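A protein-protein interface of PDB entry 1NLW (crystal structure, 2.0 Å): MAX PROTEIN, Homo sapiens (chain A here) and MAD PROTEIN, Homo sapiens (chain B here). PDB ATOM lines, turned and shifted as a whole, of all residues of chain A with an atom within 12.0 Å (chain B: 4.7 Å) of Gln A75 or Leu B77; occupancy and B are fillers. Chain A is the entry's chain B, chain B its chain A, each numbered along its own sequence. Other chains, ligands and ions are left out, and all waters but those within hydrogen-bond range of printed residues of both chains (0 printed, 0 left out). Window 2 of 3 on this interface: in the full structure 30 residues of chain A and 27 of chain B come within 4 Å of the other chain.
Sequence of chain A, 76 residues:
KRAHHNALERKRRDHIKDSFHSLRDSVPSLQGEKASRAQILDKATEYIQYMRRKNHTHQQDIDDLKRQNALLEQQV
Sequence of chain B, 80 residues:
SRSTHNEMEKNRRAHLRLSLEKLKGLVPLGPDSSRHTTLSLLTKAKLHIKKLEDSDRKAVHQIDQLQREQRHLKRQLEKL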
ATOM      1  N   ASP A  64     -18.554 -19.266   2.471  1.00  0.00           N
ATOM      2  CA  ASP A  64     -19.036 -17.911   2.232  1.00  0.00           C
ATOM      3  C   ASP A  64     -20.505 -17.773   2.634  1.00  0.00           C
ATOM      4  O   ASP A  64     -20.899 -16.774   3.229  1.00  0.00           O
ATOM      5  CB  ASP A  64     -18.867 -17.549   0.755  1.00  0.00           C
ATOM      6  CG  ASP A  64     -17.419 -17.268   0.382  1.00  0.00           C
ATOM      7  OD1 ASP A  64     -17.121 -17.179  -0.825  1.00  0.00           O
ATOM      8  OD2 ASP A  64     -16.581 -17.128   1.297  1.00  0.00           O
ATOM      9  N   LEU A  65     -21.310 -18.779   2.305  1.00  0.00           N
ATOM     10  CA  LEU A  65     -22.733 -18.766   2.639  1.00  0.00           C
ATOM     11  C   LEU A  65     -22.960 -19.011   4.122  1.00  0.00           C
ATOM     12  O   LEU A  65     -23.901 -18.480   4.709  1.00  0.00           O
ATOM     13  CB  LEU A  65     -23.486 -19.823   1.822  1.00  0.00           C
ATOM     14  CG  LEU A  65     -23.841 -19.489   0.370  1.00  0.00           C
ATOM     15  CD1 LEU A  65     -22.717 -18.716  -0.304  1.00  0.00           C
ATOM     16  CD2 LEU A  65     -24.127 -20.782  -0.376  1.00  0.00           C
ATOM     17  N   LYS A  66     -22.100 -19.821   4.730  1.00  0.00           N
ATOM     18  CA  LYS A  66     -22.232 -20.099   6.153  1.00  0.00           C
ATOM     19  C   LYS A  66     -21.959 -18.836   6.960  1.00  0.00           C
ATOM     20  O   LYS A  66     -22.665 -18.543   7.927  1.00  0.00           O
ATOM     21  CB  LYS A  66     -21.268 -21.200   6.587  1.00  0.00           C
ATOM     22  CG  LYS A  66     -21.726 -22.599   6.222  1.00  0.00           C
ATOM     23  CD  LYS A  66     -20.855 -23.656   6.885  1.00  0.00           C
ATOM     24  CE  LYS A  66     -21.378 -25.055   6.605  1.00  0.00           C
ATOM     25  NZ  LYS A  66     -20.518 -26.110   7.216  1.00  0.00           N
ATOM     26  N   ARG A  67     -20.935 -18.089   6.563  1.00  0.00           N
ATOM     27  CA  ARG A  67     -20.601 -16.871   7.277  1.00  0.00           C
ATOM     28  C   ARG A  67     -21.729 -15.871   7.085  1.00  0.00           C
ATOM     29  O   ARG A  67     -22.153 -15.206   8.033  1.00  0.00           O
ATOM     30  CB  ARG A  67     -19.277 -16.276   6.770  1.00  0.00           C
ATOM     31  CG  ARG A  67     -19.338 -15.670   5.369  1.00  0.00           C
ATOM     32  CD  ARG A  67     -18.188 -14.693   5.101  1.00  0.00           C
ATOM     33  NE  ARG A  67     -16.976 -15.300   4.543  1.00  0.00           N
ATOM     34  CZ  ARG A  67     -16.148 -16.105   5.203  1.00  0.00           C
ATOM     35  NH1 ARG A  67     -16.388 -16.427   6.467  1.00  0.00           N
ATOM     36  NH2 ARG A  67     -15.061 -16.577   4.599  1.00  0.00           N
ATOM     37  N   GLN A  68     -22.220 -15.773   5.854  1.00  0.00           N
ATOM     38  CA  GLN A  68     -23.297 -14.848   5.536  1.00  0.00           C
ATOM     39  C   GLN A  68     -24.577 -15.174   6.307  1.00  0.00           C
ATOM     40  O   GLN A  68     -25.298 -14.271   6.722  1.00  0.00           O
ATOM     41  CB  GLN A  68     -23.590 -14.867   4.034  1.00  0.00           C
ATOM     42  CG  GLN A  68     -22.444 -14.413   3.141  1.00  0.00           C
ATOM     43  CD  GLN A  68     -22.816 -14.426   1.664  1.00  0.00           C
ATOM     44  OE1 GLN A  68     -23.244 -15.449   1.127  1.00  0.00           O
ATOM     45  NE2 GLN A  68     -22.655 -13.284   1.000  1.00  0.00           N
ATOM     46  N   ASN A  69     -24.857 -16.460   6.499  1.00  0.00           N
ATOM     47  CA  ASN A  69     -26.068 -16.876   7.208  1.00  0.00           C
ATOM     48  C   ASN A  69     -25.991 -16.711   8.722  1.00  0.00           C
ATOM     49  O   ASN A  69     -26.905 -16.160   9.336  1.00  0.00           O
ATOM     50  CB  ASN A  69     -26.413 -18.330   6.878  1.00  0.00           C
ATOM     51  CG  ASN A  69     -26.994 -18.498   5.482  1.00  0.00           C
ATOM     52  OD1 ASN A  69     -27.004 -17.422   4.701  1.00  0.00           O
ATOM     53  ND2 ASN A  69     -27.426 -19.589   5.113  1.00  0.00           N
ATOM     54  N   ALA A  70     -24.909 -17.196   9.326  1.00  0.00           N
ATOM     55  CA  ALA A  70     -24.747 -17.088  10.774  1.00  0.00           C
ATOM     56  C   ALA A  70     -24.778 -15.628  11.214  1.00  0.00           C
ATOM     57  O   ALA A  70     -25.121 -15.326  12.359  1.00  0.00           O
ATOM     58  CB  ALA A  70     -23.438 -17.742  11.211  1.00  0.00           C
ATOM     59  N   LEU A  71     -24.423 -14.726  10.303  1.00  0.00           N
ATOM     60  CA  LEU A  71     -24.420 -13.298  10.599  1.00  0.00           C
ATOM     61  C   LEU A  71     -25.805 -12.683  10.423  1.00  0.00           C
ATOM     62  O   LEU A  71     -26.048 -11.551  10.846  1.00  0.00           O
ATOM     63  CB  LEU A  71     -23.411 -12.571   9.707  1.00  0.00           C
ATOM     64  CG  LEU A  71     -21.933 -12.840  10.017  1.00  0.00           C
ATOM     65  CD1 LEU A  71     -21.048 -12.133   8.997  1.00  0.00           C
ATOM     66  CD2 LEU A  71     -21.612 -12.364  11.431  1.00  0.00           C
ATOM     67  N   LEU A  72     -26.704 -13.424   9.784  1.00  0.00           N
ATOM     68  CA  LEU A  72     -28.072 -12.955   9.581  1.00  0.00           C
ATOM     69  C   LEU A  72     -28.913 -13.412  10.764  1.00  0.00           C
ATOM     70  O   LEU A  72     -29.845 -12.725  11.177  1.00  0.00           O
ATOM     71  CB  LEU A  72     -28.650 -13.512   8.275  1.00  0.00           C
ATOM     72  CG  LEU A  72     -28.595 -12.578   7.062  1.00  0.00           C
ATOM     73  CD1 LEU A  72     -27.187 -12.047   6.872  1.00  0.00           C
ATOM     74  CD2 LEU A  72     -29.064 -13.323   5.825  1.00  0.00           C
ATOM     75  N   GLU A  73     -28.575 -14.578  11.308  1.00  0.00           N
ATOM     76  CA  GLU A  73     -29.286 -15.114  12.461  1.00  0.00           C
ATOM     77  C   GLU A  73     -29.114 -14.134  13.613  1.00  0.00           C
ATOM     78  O   GLU A  73     -29.982 -14.019  14.479  1.00  0.00           O
ATOM     79  CB  GLU A  73     -28.724 -16.484  12.854  1.00  0.00           C
ATOM     80  CG  GLU A  73     -29.028 -17.597  11.861  1.00  0.00           C
ATOM     81  CD  GLU A  73     -30.513 -17.898  11.752  1.00  0.00           C
ATOM     82  OE1 GLU A  73     -30.885 -18.790  10.958  1.00  0.00           O
ATOM     83  OE2 GLU A  73     -31.310 -17.242  12.460  1.00  0.00           O
ATOM     84  N   GLN A  74     -27.982 -13.432  13.614  1.00  0.00           N
ATOM     85  CA  GLN A  74     -27.700 -12.439  14.642  1.00  0.00           C
ATOM     86  C   GLN A  74     -28.652 -11.264  14.470  1.00  0.00           C
ATOM     87  O   GLN A  74     -29.364 -10.886  15.401  1.00  0.00           O
ATOM     88  CB  GLN A  74     -26.253 -11.946  14.537  1.00  0.00           C
ATOM     89  CG  GLN A  74     -25.258 -12.743  15.366  1.00  0.00           C
ATOM     90  CD  GLN A  74     -23.874 -12.114  15.380  1.00  0.00           C
ATOM     91  OE1 GLN A  74     -23.154 -12.146  14.381  1.00  0.00           O
ATOM     92  NE2 GLN A  74     -23.502 -11.530  16.515  1.00  0.00           N
ATOM     93  N   GLN A  75     -28.660 -10.691  13.269  1.00  0.00           N
ATOM     94  CA  GLN A  75     -29.530  -9.566  12.968  1.00  0.00           C
ATOM     95  C   GLN A  75     -30.982  -9.950  13.243  1.00  0.00           C
ATOM     96  O   GLN A  75     -31.824  -9.088  13.490  1.00  0.00           O
ATOM     97  CB  GLN A  75     -29.367  -9.154  11.504  1.00  0.00           C
ATOM     98  CG  GLN A  75     -27.958  -8.716  11.144  1.00  0.00           C
ATOM     99  CD  GLN A  75     -27.813  -8.380   9.676  1.00  0.00           C
ATOM    100  OE1 GLN A  75     -28.443  -7.450   9.171  1.00  0.00           O
ATOM    101  NE2 GLN A  75     -26.982  -9.143   8.975  1.00  0.00           N
ATOM    102  N   VAL A  76     -31.261 -11.251  13.198  1.00  0.00           N
ATOM    103  CA  VAL A  76     -32.602 -11.767  13.452  1.00  0.00           C
ATOM    104  C   VAL A  76     -32.737 -12.210  14.906  1.00  0.00           C
ATOM    105  O   VAL A  76     -31.806 -11.908  15.682  1.00  0.00           O
ATOM    106  CB  VAL A  76     -32.925 -12.971  12.532  1.00  0.00           C
ATOM    107  CG1 VAL A  76     -34.240 -13.608  12.947  1.00  0.00           C
ATOM    108  CG2 VAL A  76     -33.002 -12.515  11.083  1.00  0.00           C
ATOM    109  N   LEU B  73     -33.884 -16.150   5.793  1.00  0.00           N
ATOM    110  CA  LEU B  73     -33.402 -15.198   6.794  1.00  0.00           C
ATOM    111  C   LEU B  73     -33.607 -13.765   6.299  1.00  0.00           C
ATOM    112  O   LEU B  73     -33.979 -12.872   7.071  1.00  0.00           O
ATOM    113  CB  LEU B  73     -31.918 -15.444   7.098  1.00  0.00           C
ATOM    114  CG  LEU B  73     -31.566 -16.762   7.802  1.00  0.00           C
ATOM    115  CD1 LEU B  73     -30.045 -16.961   7.851  1.00  0.00           C
ATOM    116  CD2 LEU B  73     -32.147 -16.732   9.207  1.00  0.00           C
ATOM    117  N   LYS B  74     -33.367 -13.542   5.014  1.00  0.00           N
ATOM    118  CA  LYS B  74     -33.553 -12.212   4.450  1.00  0.00           C
ATOM    119  C   LYS B  74     -35.015 -11.770   4.541  1.00  0.00           C
ATOM    120  O   LYS B  74     -35.306 -10.675   5.014  1.00  0.00           O
ATOM    121  CB  LYS B  74     -33.113 -12.182   2.989  1.00  0.00           C
ATOM    122  CG  LYS B  74     -31.622 -12.357   2.767  1.00  0.00           C
ATOM    123  CD  LYS B  74     -30.834 -11.098   3.089  1.00  0.00           C
ATOM    124  CE  LYS B  74     -29.392 -11.236   2.619  1.00  0.00           C
ATOM    125  NZ  LYS B  74     -28.572 -10.051   2.988  1.00  0.00           N
ATOM    126  N   ARG B  75     -35.930 -12.619   4.081  1.00  0.00           N
ATOM    127  CA  ARG B  75     -37.355 -12.295   4.110  1.00  0.00           C
ATOM    128  C   ARG B  75     -37.843 -12.088   5.530  1.00  0.00           C
ATOM    129  O   ARG B  75     -38.684 -11.228   5.799  1.00  0.00           O
ATOM    130  CB  ARG B  75     -38.171 -13.398   3.426  1.00  0.00           C
ATOM    131  CG  ARG B  75     -38.117 -13.338   1.902  1.00  0.00           C
ATOM    132  CD  ARG B  75     -38.974 -14.412   1.221  1.00  0.00           C
ATOM    133  NE  ARG B  75     -38.292 -15.703   1.124  1.00  0.00           N
ATOM    134  CZ  ARG B  75     -38.612 -16.768   1.848  1.00  0.00           C
ATOM    135  NH1 ARG B  75     -39.606 -16.692   2.720  1.00  0.00           N
ATOM    136  NH2 ARG B  75     -37.943 -17.904   1.702  1.00  0.00           N
ATOM    137  N   GLN B  76     -37.301 -12.886   6.440  1.00  0.00           N
ATOM    138  CA  GLN B  76     -37.657 -12.803   7.841  1.00  0.00           C
ATOM    139  C   GLN B  76     -37.171 -11.466   8.386  1.00  0.00           C
ATOM    140  O   GLN B  76     -37.922 -10.726   9.024  1.00  0.00           O
ATOM    141  CB  GLN B  76     -37.001 -13.959   8.595  1.00  0.00           C
ATOM    142  CG  GLN B  76     -37.357 -14.040  10.059  1.00  0.00           C
ATOM    143  CD  GLN B  76     -36.908 -15.346  10.684  1.00  0.00           C
ATOM    144  OE1 GLN B  76     -35.741 -15.731  10.572  1.00  0.00           O
ATOM    145  NE2 GLN B  76     -37.832 -16.035  11.349  1.00  0.00           N
ATOM    146  N   LEU B  77     -35.910 -11.157   8.106  1.00  0.00           N
ATOM    147  CA  LEU B  77     -35.296  -9.918   8.558  1.00  0.00           C
ATOM    148  C   LEU B  77     -36.133  -8.705   8.154  1.00  0.00           C
ATOM    149  O   LEU B  77     -36.001  -7.626   8.734  1.00  0.00           O
ATOM    150  CB  LEU B  77     -33.888  -9.805   7.975  1.00  0.00           C
ATOM    151  CG  LEU B  77     -32.901  -8.922   8.735  1.00  0.00           C
ATOM    152  CD1 LEU B  77     -32.818  -9.373  10.182  1.00  0.00           C
ATOM    153  CD2 LEU B  77     -31.538  -9.007   8.071  1.00  0.00           C
ATOM    154  N   GLU B  78     -36.995  -8.884   7.160  1.00  0.00           N
ATOM    155  CA  GLU B  78     -37.855  -7.798   6.708  1.00  0.00           C
ATOM    156  C   GLU B  78     -38.862  -7.487   7.804  1.00  0.00           C
ATOM    157  O   GLU B  78     -39.017  -6.336   8.212  1.00  0.00           O
ATOM    158  CB  GLU B  78     -38.602  -8.191   5.431  1.00  0.00           C
ATOM    159  CG  GLU B  78     -37.705  -8.689   4.322  1.00  0.00           C
ATOM    160  CD  GLU B  78     -36.561  -7.741   4.045  1.00  0.00           C
ATOM    161  OE1 GLU B  78     -36.822  -6.601   3.609  1.00  0.00           O
ATOM    162  OE2 GLU B  78     -35.399  -8.135   4.273  1.00  0.00           O
ATOM    163  N   LYS B  79     -39.544  -8.521   8.284  1.00  0.00           N
ATOM    164  CA  LYS B  79     -40.535  -8.351   9.335  1.00  0.00           C
ATOM    165  C   LYS B  79     -39.866  -8.126  10.691  1.00  0.00           C
ATOM    166  O   LYS B  79     -39.012  -7.215  10.772  1.00  0.00           O
ATOM    167  CB  LYS B  79     -41.438  -9.572   9.392  1.00  0.00           C
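O of Lys B74 sits close to OE2 of Glu B78 (2.6 Å).
OD1 of Asn A69 lies close to O of Leu A65.
The side-chain amide nitrogen of Gln A75 lies within hydrogen-bond range of the backbone carbonyl oxygen of Leu A71 (3.2 Å).
Leu B73 touches Asn A69.
Leu B73 touches Leu A72.
CD2 of Leu A72 touches CE of Lys B74, at 3.8 Å.
Glu A73 touches Leu B73.
O of Gln A75 touches CD1 of Leu B77, 3.5 Å away.
CG1 of Val A76 touches OE1 of Gln B76 (3.5 Å).
CG2 of Val A76 touches CD1 of Leu B77 (3.3 Å).
Printed residues of chain B within 4 Å of Asn A69: Leu B73.
Of the printed residues of chain B, Leu A72 touches Leu B73 and Lys B74.
Of the printed residues of chain B, Gln A75 touches Leu B77 (3.5 Å).
Printed residues of chain B within 4 Å of Val A76: Gln B76 and Leu B77.
Printed residues of chain A within 4 Å of Leu B73: Asn A69, Leu A72 and Glu A73.
Lys B74 touches one residue of chain A.
Printed residues of chain A within 4 Å of Gln B76: Val A76 (3.5 Å).
Leu B77 touches two residues of chain A.
Glu B78 touches none of the printed residues of chain A.
No residue of chain A comes within 4 Å of Lys B79.
The nearest printed residue of chain B that does not touch Gln A75 is Lys B74 (6.3 Å).
The nearest printed residue of chain B that does not touch Glu A73 is Gln B76 (5.0 Å).
Printed residues of chain A that touch a printed residue of chain B: Asn A69, Leu A72, Glu A73, Gln A75 and Val A76.
Hydrophobic or aromatic side chains of chain B that line the printed part of chain A: Leu B73 and Leu B77.
Along chain B the printed residues that touch a printed residue of chain A span positions 73 to 77.
Among the printed residues, 7 pairs touch across the chains.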
